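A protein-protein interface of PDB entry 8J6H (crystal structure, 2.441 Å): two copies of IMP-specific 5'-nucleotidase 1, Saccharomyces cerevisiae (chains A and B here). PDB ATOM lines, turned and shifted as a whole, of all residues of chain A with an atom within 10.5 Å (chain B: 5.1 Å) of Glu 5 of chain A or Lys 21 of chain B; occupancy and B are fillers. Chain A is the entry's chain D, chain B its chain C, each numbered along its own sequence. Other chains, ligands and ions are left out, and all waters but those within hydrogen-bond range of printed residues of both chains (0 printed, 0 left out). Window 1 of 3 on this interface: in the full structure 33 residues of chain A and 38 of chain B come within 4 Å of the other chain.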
ATOM      1  N   ARG A   1      -8.414  19.147  -9.393  1.00  0.00           N
ATOM      2  CA  ARG A   1      -8.068  20.478  -9.877  1.00  0.00           C
ATOM      3  C   ARG A   1      -9.240  21.135 -10.591  1.00  0.00           C
ATOM      4  O   ARG A   1      -9.788  20.578 -11.542  1.00  0.00           O
ATOM      5  CB  ARG A   1      -6.865  20.411 -10.817  1.00  0.00           C
ATOM      6  CG  ARG A   1      -6.318  21.772 -11.204  1.00  0.00           C
ATOM      7  CD  ARG A   1      -5.256  21.658 -12.281  1.00  0.00           C
ATOM      8  NE  ARG A   1      -5.700  20.875 -13.432  1.00  0.00           N
ATOM      9  CZ  ARG A   1      -6.206  21.402 -14.544  1.00  0.00           C
ATOM     10  NH1 ARG A   1      -6.579  20.616 -15.544  1.00  0.00           N
ATOM     11  NH2 ARG A   1      -6.343  22.715 -14.655  1.00  0.00           N
ATOM     12  N   TYR A   2      -9.623  22.322 -10.131  1.00  0.00           N
ATOM     13  CA  TYR A   2     -10.683  23.079 -10.785  1.00  0.00           C
ATOM     14  C   TYR A   2     -10.191  23.596 -12.132  1.00  0.00           C
ATOM     15  O   TYR A   2      -9.489  24.605 -12.202  1.00  0.00           O
ATOM     16  CB  TYR A   2     -11.152  24.241  -9.906  1.00  0.00           C
ATOM     17  CG  TYR A   2     -12.375  24.958 -10.439  1.00  0.00           C
ATOM     18  CD1 TYR A   2     -13.651  24.587 -10.034  1.00  0.00           C
ATOM     19  CD2 TYR A   2     -12.255  26.005 -11.345  1.00  0.00           C
ATOM     20  CE1 TYR A   2     -14.772  25.237 -10.518  1.00  0.00           C
ATOM     21  CE2 TYR A   2     -13.370  26.659 -11.834  1.00  0.00           C
ATOM     22  CZ  TYR A   2     -14.626  26.272 -11.417  1.00  0.00           C
ATOM     23  OH  TYR A   2     -15.738  26.922 -11.901  1.00  0.00           O
ATOM     24  N   ARG A   3     -10.559  22.891 -13.196  1.00  0.00           N
ATOM     25  CA  ARG A   3     -10.159  23.267 -14.545  1.00  0.00           C
ATOM     26  C   ARG A   3     -10.782  24.598 -14.950  1.00  0.00           C
ATOM     27  O   ARG A   3     -11.974  24.672 -15.250  1.00  0.00           O
ATOM     28  CB  ARG A   3     -10.547  22.171 -15.537  1.00  0.00           C
ATOM     29  CG  ARG A   3      -9.871  20.838 -15.271  1.00  0.00           C
ATOM     30  CD  ARG A   3     -10.605  19.697 -15.952  1.00  0.00           C
ATOM     31  NE  ARG A   3     -11.965  19.547 -15.441  1.00  0.00           N
ATOM     32  CZ  ARG A   3     -12.806  18.594 -15.825  1.00  0.00           C
ATOM     33  NH1 ARG A   3     -14.025  18.535 -15.306  1.00  0.00           N
ATOM     34  NH2 ARG A   3     -12.429  17.698 -16.728  1.00  0.00           N
ATOM     35  N   VAL A   4      -9.964  25.646 -14.957  1.00  0.00           N
ATOM     36  CA  VAL A   4     -10.435  26.991 -15.269  1.00  0.00           C
ATOM     37  C   VAL A   4     -10.713  27.181 -16.758  1.00  0.00           C
ATOM     38  O   VAL A   4     -11.219  28.224 -17.173  1.00  0.00           O
ATOM     39  CB  VAL A   4      -9.414  28.055 -14.817  1.00  0.00           C
ATOM     40  CG1 VAL A   4      -9.343  28.115 -13.298  1.00  0.00           C
ATOM     41  CG2 VAL A   4      -8.044  27.764 -15.413  1.00  0.00           C
ATOM     42  N   GLU A   5     -10.385  26.170 -17.557  1.00  0.00           N
ATOM     43  CA  GLU A   5     -10.530  26.260 -19.007  1.00  0.00           C
ATOM     44  C   GLU A   5     -11.618  25.328 -19.533  1.00  0.00           C
ATOM     45  O   GLU A   5     -11.799  25.195 -20.743  1.00  0.00           O
ATOM     46  CB  GLU A   5      -9.198  25.937 -19.694  1.00  0.00           C
ATOM     47  CG  GLU A   5      -8.844  24.451 -19.728  1.00  0.00           C
ATOM     48  CD  GLU A   5      -8.421  23.901 -18.376  1.00  0.00           C
ATOM     49  OE1 GLU A   5      -8.234  24.697 -17.433  1.00  0.00           O
ATOM     50  OE2 GLU A   5      -8.274  22.665 -18.261  1.00  0.00           O
ATOM     51  N   TYR A   6     -12.343  24.696 -18.613  1.00  0.00           N
ATOM     52  CA  TYR A   6     -13.335  23.677 -18.953  1.00  0.00           C
ATOM     53  C   TYR A   6     -14.409  24.167 -19.923  1.00  0.00           C
ATOM     54  O   TYR A   6     -14.709  23.503 -20.915  1.00  0.00           O
ATOM     55  CB  TYR A   6     -13.999  23.156 -17.674  1.00  0.00           C
ATOM     56  CG  TYR A   6     -14.935  21.986 -17.885  1.00  0.00           C
ATOM     57  CD1 TYR A   6     -14.441  20.700 -18.066  1.00  0.00           C
ATOM     58  CD2 TYR A   6     -16.313  22.164 -17.890  1.00  0.00           C
ATOM     59  CE1 TYR A   6     -15.291  19.627 -18.255  1.00  0.00           C
ATOM     60  CE2 TYR A   6     -17.171  21.096 -18.077  1.00  0.00           C
ATOM     61  CZ  TYR A   6     -16.655  19.829 -18.259  1.00  0.00           C
ATOM     62  OH  TYR A   6     -17.503  18.762 -18.446  1.00  0.00           O
ATOM     63  N   HIS A   7     -14.979  25.333 -19.638  1.00  0.00           N
ATOM     64  CA  HIS A   7     -16.134  25.823 -20.385  1.00  0.00           C
ATOM     65  C   HIS A   7     -15.773  26.436 -21.737  1.00  0.00           C
ATOM     66  O   HIS A   7     -16.657  26.809 -22.509  1.00  0.00           O
ATOM     67  CB  HIS A   7     -16.900  26.843 -19.543  1.00  0.00           C
ATOM     68  CG  HIS A   7     -17.360  26.308 -18.223  1.00  0.00           C
ATOM     69  ND1 HIS A   7     -18.547  25.625 -18.071  1.00  0.00           N
ATOM     70  CD2 HIS A   7     -16.788  26.348 -16.997  1.00  0.00           C
ATOM     71  CE1 HIS A   7     -18.689  25.271 -16.806  1.00  0.00           C
ATOM     72  NE2 HIS A   7     -17.635  25.697 -16.133  1.00  0.00           N
ATOM     73  N   LEU A   8     -14.481  26.534 -22.028  1.00  0.00           N
ATOM     74  CA  LEU A   8     -14.038  27.068 -23.311  1.00  0.00           C
ATOM     75  C   LEU A   8     -14.202  26.044 -24.426  1.00  0.00           C
ATOM     76  O   LEU A   8     -14.195  26.392 -25.608  1.00  0.00           O
ATOM     77  CB  LEU A   8     -12.582  27.521 -23.234  1.00  0.00           C
ATOM     78  CG  LEU A   8     -12.329  28.856 -22.539  1.00  0.00           C
ATOM     79  CD1 LEU A   8     -10.913  29.304 -22.813  1.00  0.00           C
ATOM     80  CD2 LEU A   8     -13.328  29.907 -23.003  1.00  0.00           C
ATOM     81  N   LYS A   9     -14.347  24.781 -24.044  1.00  0.00           N
ATOM     82  CA  LYS A   9     -14.497  23.702 -25.012  1.00  0.00           C
ATOM     83  C   LYS A   9     -15.773  22.903 -24.784  1.00  0.00           C
ATOM     84  O   LYS A   9     -16.366  22.946 -23.707  1.00  0.00           O
ATOM     85  CB  LYS A   9     -13.293  22.762 -24.959  1.00  0.00           C
ATOM     86  CG  LYS A   9     -12.071  23.259 -25.715  1.00  0.00           C
ATOM     87  CD  LYS A   9     -10.861  22.358 -25.488  1.00  0.00           C
ATOM     88  CE  LYS A   9     -11.255  21.003 -24.914  1.00  0.00           C
ATOM     89  NZ  LYS A   9     -10.069  20.151 -24.633  1.00  0.00           N
ATOM     90  N   SER A  10     -16.182  22.170 -25.813  1.00  0.00           N
ATOM     91  CA  SER A  10     -17.342  21.296 -25.723  1.00  0.00           C
ATOM     92  C   SER A  10     -16.988  20.017 -24.972  1.00  0.00           C
ATOM     93  O   SER A  10     -16.104  19.270 -25.388  1.00  0.00           O
ATOM     94  CB  SER A  10     -17.869  20.958 -27.120  1.00  0.00           C
ATOM     95  OG  SER A  10     -17.853  22.099 -27.961  1.00  0.00           O
ATOM     96  N   HIS A  11     -17.672  19.773 -23.858  1.00  0.00           N
ATOM     97  CA  HIS A  11     -17.454  18.556 -23.082  1.00  0.00           C
ATOM     98  C   HIS A  11     -18.753  17.756 -22.926  1.00  0.00           C
ATOM     99  O   HIS A  11     -19.033  17.210 -21.859  1.00  0.00           O
ATOM    100  CB  HIS A  11     -16.860  18.893 -21.710  1.00  0.00           C
ATOM    101  CG  HIS A  11     -15.428  19.335 -21.760  1.00  0.00           C
ATOM    102  ND1 HIS A  11     -15.059  20.656 -21.902  1.00  0.00           N
ATOM    103  CD2 HIS A  11     -14.274  18.629 -21.690  1.00  0.00           C
ATOM    104  CE1 HIS A  11     -13.741  20.745 -21.913  1.00  0.00           C
ATOM    105  NE2 HIS A  11     -13.241  19.529 -21.786  1.00  0.00           N
ATOM    106  N   GLU A 341      -5.093  19.913 -31.668  1.00  0.00           N
ATOM    107  CA  GLU A 341      -5.394  21.155 -30.956  1.00  0.00           C
ATOM    108  C   GLU A 341      -5.567  22.347 -31.894  1.00  0.00           C
ATOM    109  O   GLU A 341      -6.369  23.243 -31.629  1.00  0.00           O
ATOM    110  CB  GLU A 341      -4.293  21.468 -29.937  1.00  0.00           C
ATOM    111  CG  GLU A 341      -4.160  20.460 -28.805  1.00  0.00           C
ATOM    112  CD  GLU A 341      -3.314  19.259 -29.184  1.00  0.00           C
ATOM    113  OE1 GLU A 341      -2.912  19.160 -30.361  1.00  0.00           O
ATOM    114  OE2 GLU A 341      -3.041  18.418 -28.301  1.00  0.00           O
ATOM    115  N   GLU A 344      -9.037  22.070 -33.428  1.00  0.00           N
ATOM    116  CA  GLU A 344     -10.065  22.469 -32.470  1.00  0.00           C
ATOM    117  C   GLU A 344     -10.070  23.979 -32.274  1.00  0.00           C
ATOM    118  O   GLU A 344     -11.127  24.581 -32.090  1.00  0.00           O
ATOM    119  CB  GLU A 344      -9.867  21.766 -31.125  1.00  0.00           C
ATOM    120  CG  GLU A 344      -9.132  20.445 -31.216  1.00  0.00           C
ATOM    121  CD  GLU A 344      -9.272  19.607 -29.964  1.00  0.00           C
ATOM    122  OE1 GLU A 344     -10.364  19.623 -29.355  1.00  0.00           O
ATOM    123  OE2 GLU A 344      -8.286  18.942 -29.580  1.00  0.00           O
ATOM    124  N   LEU A 348     -13.600  26.032 -33.040  1.00  0.00           N
ATOM    125  CA  LEU A 348     -14.074  26.816 -31.904  1.00  0.00           C
ATOM    126  C   LEU A 348     -14.079  28.296 -32.256  1.00  0.00           C
ATOM    127  O   LEU A 348     -15.005  29.028 -31.905  1.00  0.00           O
ATOM    128  CB  LEU A 348     -13.208  26.567 -30.670  1.00  0.00           C
ATOM    129  CG  LEU A 348     -13.460  25.261 -29.916  1.00  0.00           C
ATOM    130  CD1 LEU A 348     -12.355  25.011 -28.904  1.00  0.00           C
ATOM    131  CD2 LEU A 348     -14.818  25.293 -29.234  1.00  0.00           C
ATOM    132  N   ILE B  17       1.738  15.838 -14.953  1.00  0.00           N
ATOM    133  CA  ILE B  17       1.338  16.466 -16.207  1.00  0.00           C
ATOM    134  C   ILE B  17       0.078  17.312 -16.034  1.00  0.00           C
ATOM    135  O   ILE B  17      -0.014  18.416 -16.572  1.00  0.00           O
ATOM    136  CB  ILE B  17       1.107  15.416 -17.309  1.00  0.00           C
ATOM    137  CG1 ILE B  17       2.384  14.605 -17.540  1.00  0.00           C
ATOM    138  CG2 ILE B  17       0.668  16.085 -18.602  1.00  0.00           C
ATOM    139  CD1 ILE B  17       2.298  13.639 -18.701  1.00  0.00           C
ATOM    140  N   ASP B  18      -0.889  16.797 -15.279  1.00  0.00           N
ATOM    141  CA  ASP B  18      -2.106  17.552 -14.993  1.00  0.00           C
ATOM    142  C   ASP B  18      -1.788  18.775 -14.141  1.00  0.00           C
ATOM    143  O   ASP B  18      -2.430  19.817 -14.268  1.00  0.00           O
ATOM    144  CB  ASP B  18      -3.142  16.674 -14.288  1.00  0.00           C
ATOM    145  CG  ASP B  18      -4.400  17.442 -13.918  1.00  0.00           C
ATOM    146  OD1 ASP B  18      -5.139  17.856 -14.836  1.00  0.00           O
ATOM    147  OD2 ASP B  18      -4.648  17.634 -12.708  1.00  0.00           O
ATOM    148  N   TRP B  19      -0.790  18.635 -13.274  1.00  0.00           N
ATOM    149  CA  TRP B  19      -0.334  19.736 -12.433  1.00  0.00           C
ATOM    150  C   TRP B  19       0.219  20.870 -13.288  1.00  0.00           C
ATOM    151  O   TRP B  19      -0.116  22.036 -13.080  1.00  0.00           O
ATOM    152  CB  TRP B  19       0.724  19.246 -11.442  1.00  0.00           C
ATOM    153  CG  TRP B  19       1.244  20.306 -10.519  1.00  0.00           C
ATOM    154  CD1 TRP B  19       0.548  20.952  -9.539  1.00  0.00           C
ATOM    155  CD2 TRP B  19       2.578  20.830 -10.475  1.00  0.00           C
ATOM    156  NE1 TRP B  19       1.363  21.852  -8.895  1.00  0.00           N
ATOM    157  CE2 TRP B  19       2.614  21.796  -9.450  1.00  0.00           C
ATOM    158  CE3 TRP B  19       3.742  20.579 -11.207  1.00  0.00           C
ATOM    159  CZ2 TRP B  19       3.768  22.512  -9.139  1.00  0.00           C
ATOM    160  CZ3 TRP B  19       4.887  21.290 -10.896  1.00  0.00           C
ATOM    161  CH2 TRP B  19       4.892  22.244  -9.871  1.00  0.00           C
ATOM    162  N   VAL B  20       1.062  20.519 -14.256  1.00  0.00           N
ATOM    163  CA  VAL B  20       1.632  21.497 -15.177  1.00  0.00           C
ATOM    164  C   VAL B  20       0.542  22.150 -16.022  1.00  0.00           C
ATOM    165  O   VAL B  20       0.570  23.357 -16.265  1.00  0.00           O
ATOM    166  CB  VAL B  20       2.683  20.852 -16.106  1.00  0.00           C
ATOM    167  CG1 VAL B  20       3.230  21.877 -17.086  1.00  0.00           C
ATOM    168  CG2 VAL B  20       3.811  20.247 -15.289  1.00  0.00           C
ATOM    169  N   LYS B  21      -0.419  21.342 -16.460  1.00  0.00           N
ATOM    170  CA  LYS B  21      -1.537  21.829 -17.261  1.00  0.00           C
ATOM    171  C   LYS B  21      -2.338  22.883 -16.505  1.00  0.00           C
ATOM    172  O   LYS B  21      -2.795  23.866 -17.088  1.00  0.00           O
ATOM    173  CB  LYS B  21      -2.443  20.665 -17.672  1.00  0.00           C
ATOM    174  CG  LYS B  21      -3.526  21.027 -18.679  1.00  0.00           C
ATOM    175  CD  LYS B  21      -3.948  19.805 -19.483  1.00  0.00           C
ATOM    176  CE  LYS B  21      -5.422  19.855 -19.856  1.00  0.00           C
ATOM    177  NZ  LYS B  21      -5.817  21.168 -20.434  1.00  0.00           N
ATOM    178  N   GLY B  22      -2.498  22.675 -15.203  1.00  0.00           N
ATOM    179  CA  GLY B  22      -3.206  23.619 -14.361  1.00  0.00           C
ATOM    180  C   GLY B  22      -2.451  24.922 -14.199  1.00  0.00           C
ATOM    181  O   GLY B  22      -3.047  25.999 -14.188  1.00  0.00           O
ATOM    182  N   LEU B  23      -1.132  24.821 -14.070  1.00  0.00           N
ATOM    183  CA  LEU B  23      -0.282  25.999 -13.958  1.00  0.00           C
ATOM    184  C   LEU B  23      -0.288  26.796 -15.257  1.00  0.00           C
ATOM    185  O   LEU B  23      -0.200  28.020 -15.244  1.00  0.00           O
ATOM    186  CB  LEU B  23       1.150  25.600 -13.596  1.00  0.00           C
ATOM    187  CG  LEU B  23       1.339  24.795 -12.309  1.00  0.00           C
ATOM    188  CD1 LEU B  23       2.775  24.307 -12.189  1.00  0.00           C
ATOM    189  CD2 LEU B  23       0.944  25.622 -11.096  1.00  0.00           C
ATOM    190  N   LEU B  24      -0.393  26.086 -16.376  1.00  0.00           N
ATOM    191  CA  LEU B  24      -0.369  26.709 -17.695  1.00  0.00           C
ATOM    192  C   LEU B  24      -1.720  27.306 -18.079  1.00  0.00           C
ATOM    193  O   LEU B  24      -1.793  28.219 -18.900  1.00  0.00           O
ATOM    194  CB  LEU B  24       0.067  25.690 -18.751  1.00  0.00           C
ATOM    195  CG  LEU B  24       1.530  25.711 -19.201  1.00  0.00           C
ATOM    196  CD1 LEU B  24       2.456  26.157 -18.080  1.00  0.00           C
ATOM    197  CD2 LEU B  24       1.944  24.346 -19.740  1.00  0.00           C
ATOM    198  N   ALA B  25      -2.787  26.785 -17.480  1.00  0.00           N
ATOM    199  CA  ALA B  25      -4.140  27.207 -17.824  1.00  0.00           C
ATOM    200  C   ALA B  25      -4.471  28.592 -17.273  1.00  0.00           C
ATOM    201  O   ALA B  25      -5.256  29.330 -17.869  1.00  0.00           O
ATOM    202  CB  ALA B  25      -5.151  26.188 -17.321  1.00  0.00           C
ATOM    203  N   PHE B  28      -3.276  31.229 -19.508  1.00  0.00           N
ATOM    204  CA  PHE B  28      -4.054  31.031 -20.724  1.00  0.00           C
ATOM    205  C   PHE B  28      -5.407  31.729 -20.640  1.00  0.00           C
ATOM    206  O   PHE B  28      -5.758  32.523 -21.507  1.00  0.00           O
ATOM    207  CB  PHE B  28      -4.254  29.538 -21.003  1.00  0.00           C
ATOM    208  CG  PHE B  28      -5.195  29.256 -22.144  1.00  0.00           C
ATOM    209  CD1 PHE B  28      -6.484  28.812 -21.902  1.00  0.00           C
ATOM    210  CD2 PHE B  28      -4.793  29.438 -23.456  1.00  0.00           C
ATOM    211  CE1 PHE B  28      -7.353  28.555 -22.946  1.00  0.00           C
ATOM    212  CE2 PHE B  28      -5.656  29.186 -24.505  1.00  0.00           C
ATOM    213  CZ  PHE B  28      -6.938  28.743 -24.249  1.00  0.00           C
ATOM    214  N   VAL B  29      -6.165  31.440 -19.589  1.00  0.00           N
ATOM    215  CA  VAL B  29      -7.505  32.001 -19.465  1.00  0.00           C
ATOM    216  C   VAL B  29      -7.472  33.513 -19.247  1.00  0.00           C
ATOM    217  O   VAL B  29      -8.360  34.230 -19.710  1.00  0.00           O
ATOM    218  CB  VAL B  29      -8.297  31.328 -18.327  1.00  0.00           C
ATOM    219  CG1 VAL B  29      -8.521  29.858 -18.643  1.00  0.00           C
ATOM    220  CG2 VAL B  29      -7.574  31.480 -17.003  1.00  0.00           C
ATOM    221  N   ALA B 133      -6.456  25.439 -24.672  1.00  0.00           N
ATOM    222  CA  ALA B 133      -5.390  25.513 -23.678  1.00  0.00           C
ATOM    223  C   ALA B 133      -4.268  24.522 -23.991  1.00  0.00           C
ATOM    224  O   ALA B 133      -4.470  23.585 -24.765  1.00  0.00           O
ATOM    225  CB  ALA B 133      -5.960  25.253 -22.286  1.00  0.00           C
ATOM    226  N   PRO B 134      -3.074  24.739 -23.407  1.00  0.00           N
ATOM    227  CA  PRO B 134      -1.993  23.752 -23.518  1.00  0.00           C
ATOM    228  C   PRO B 134      -2.461  22.356 -23.119  1.00  0.00           C
ATOM    229  O   PRO B 134      -2.940  22.159 -22.001  1.00  0.00           O
ATOM    230  CB  PRO B 134      -0.938  24.281 -22.546  1.00  0.00           C
ATOM    231  CG  PRO B 134      -1.142  25.754 -22.561  1.00  0.00           C
ATOM    232  CD  PRO B 134      -2.623  25.970 -22.730  1.00  0.00           C
ATOM    233  N   SER B 135      -2.327  21.403 -24.035  1.00  0.00           N
ATOM    234  CA  SER B 135      -2.908  20.078 -23.853  1.00  0.00           C
ATOM    235  C   SER B 135      -2.001  19.122 -23.091  1.00  0.00           C
ATOM    236  O   SER B 135      -0.838  19.425 -22.823  1.00  0.00           O
ATOM    237  CB  SER B 135      -3.257  19.471 -25.212  1.00  0.00           C
ATOM    238  OG  SER B 135      -2.096  18.980 -25.861  1.00  0.00           O
ATOM    239  N   PHE B 136      -2.556  17.966 -22.742  1.00  0.00           N
ATOM    240  CA  PHE B 136      -1.791  16.883 -22.141  1.00  0.00           C
ATOM    241  C   PHE B 136      -0.724  16.395 -23.115  1.00  0.00           C
ATOM    242  O   PHE B 136       0.406  16.107 -22.722  1.00  0.00           O
ATOM    243  CB  PHE B 136      -2.725  15.736 -21.734  1.00  0.00           C
ATOM    244  CG  PHE B 136      -2.053  14.393 -21.664  1.00  0.00           C
ATOM    245  CD1 PHE B 136      -2.108  13.519 -22.739  1.00  0.00           C
ATOM    246  CD2 PHE B 136      -1.378  13.999 -20.522  1.00  0.00           C
ATOM    247  CE1 PHE B 136      -1.493  12.284 -22.678  1.00  0.00           C
ATOM    248  CE2 PHE B 136      -0.762  12.763 -20.455  1.00  0.00           C
ATOM    249  CZ  PHE B 136      -0.820  11.904 -21.534  1.00  0.00           C
ATOM    250  N   ILE B 139       2.233  18.946 -23.329  1.00  0.00           N
ATOM    251  CA  ILE B 139       3.149  18.784 -22.209  1.00  0.00           C
ATOM    252  C   ILE B 139       3.940  17.484 -22.322  1.00  0.00           C
ATOM    253  O   ILE B 139       5.136  17.448 -22.031  1.00  0.00           O
ATOM    254  CB  ILE B 139       2.391  18.812 -20.872  1.00  0.00           C
ATOM    255  CG1 ILE B 139       1.583  20.106 -20.758  1.00  0.00           C
ATOM    256  CG2 ILE B 139       3.353  18.680 -19.701  1.00  0.00           C
ATOM    257  CD1 ILE B 139       0.528  20.071 -19.685  1.00  0.00           C
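Among the printed residues, merely in contact across the chains: Arg 1 of chain A with Gly 22 of chain B, Glu 5 of chain A with Ala 25 of chain B, Val 4 of chain A with Val 29 of chain B, Leu 8 of chain A with Phe 28 of chain B, Val 4 of chain A with Ala 25 of chain B and Glu 5 of chain A with Ala 133 of chain B.
The side-chain carboxylate of Asp 18 of chain B is in salt-bridge range of the guanidinium group of Arg 1 of chain A, at 3.2 Å.
The side-chain carboxylate (OE2) of Glu 5 of chain A is in salt-bridge range of the side-chain amino group (NZ) of Lys 21 of chain B, 3.6 Å away.
OG of Ser 135 of chain B is in hydrogen-bond range of OE2 of Glu 341 of chain A (2.7 Å).
Of the 16 printed residues of chain B, 8 touch a printed residue of chain A.
Printed residues of chain B that touch a printed residue of chain A: Asp 18, Lys 21, Gly 22, Ala 25, Phe 28, Val 29, Ala 133 and Ser 135.
Hydrophobic or aromatic side chains of chain B that line the printed part of chain A: Ala 25, Phe 28, Val 29 and Ala 133.
Of the 14 printed residues of chain A, 5 touch a printed residue of chain B.
Printed residues of chain A that touch a printed residue of chain B: Arg 1, Val 4, Glu 5, Leu 8 and Glu 341.
O of Pro 134 of chain B is in hydrogen-bond range of NZ of Lys 21 of chain B.
NH1 of Arg 1 of chain A is in salt-bridge range of OE2 of Glu 5 of chain A.
Glu 5 of chain A touches three residues of chain B.
Printed residues of chain B within 4 Å of Glu 341 of chain A: Ser 135 (2.7 Å).
Asp 18 of chain B touches one residue of chain A.
No residue of chain A comes within 4 Å of Val 20 of chain B.
Ala 25 of chain B touches just these residues of chain A: Val 4 (3.8 Å) and Glu 5 (3.4 Å).
Printed residues of chain A within 4 Å of Val 29 of chain B: Val 4.
The nearest residue of chain A that does not touch Lys 21 of chain B is Arg 1 of chain A (4.4 Å).
No position is printed for both chains.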
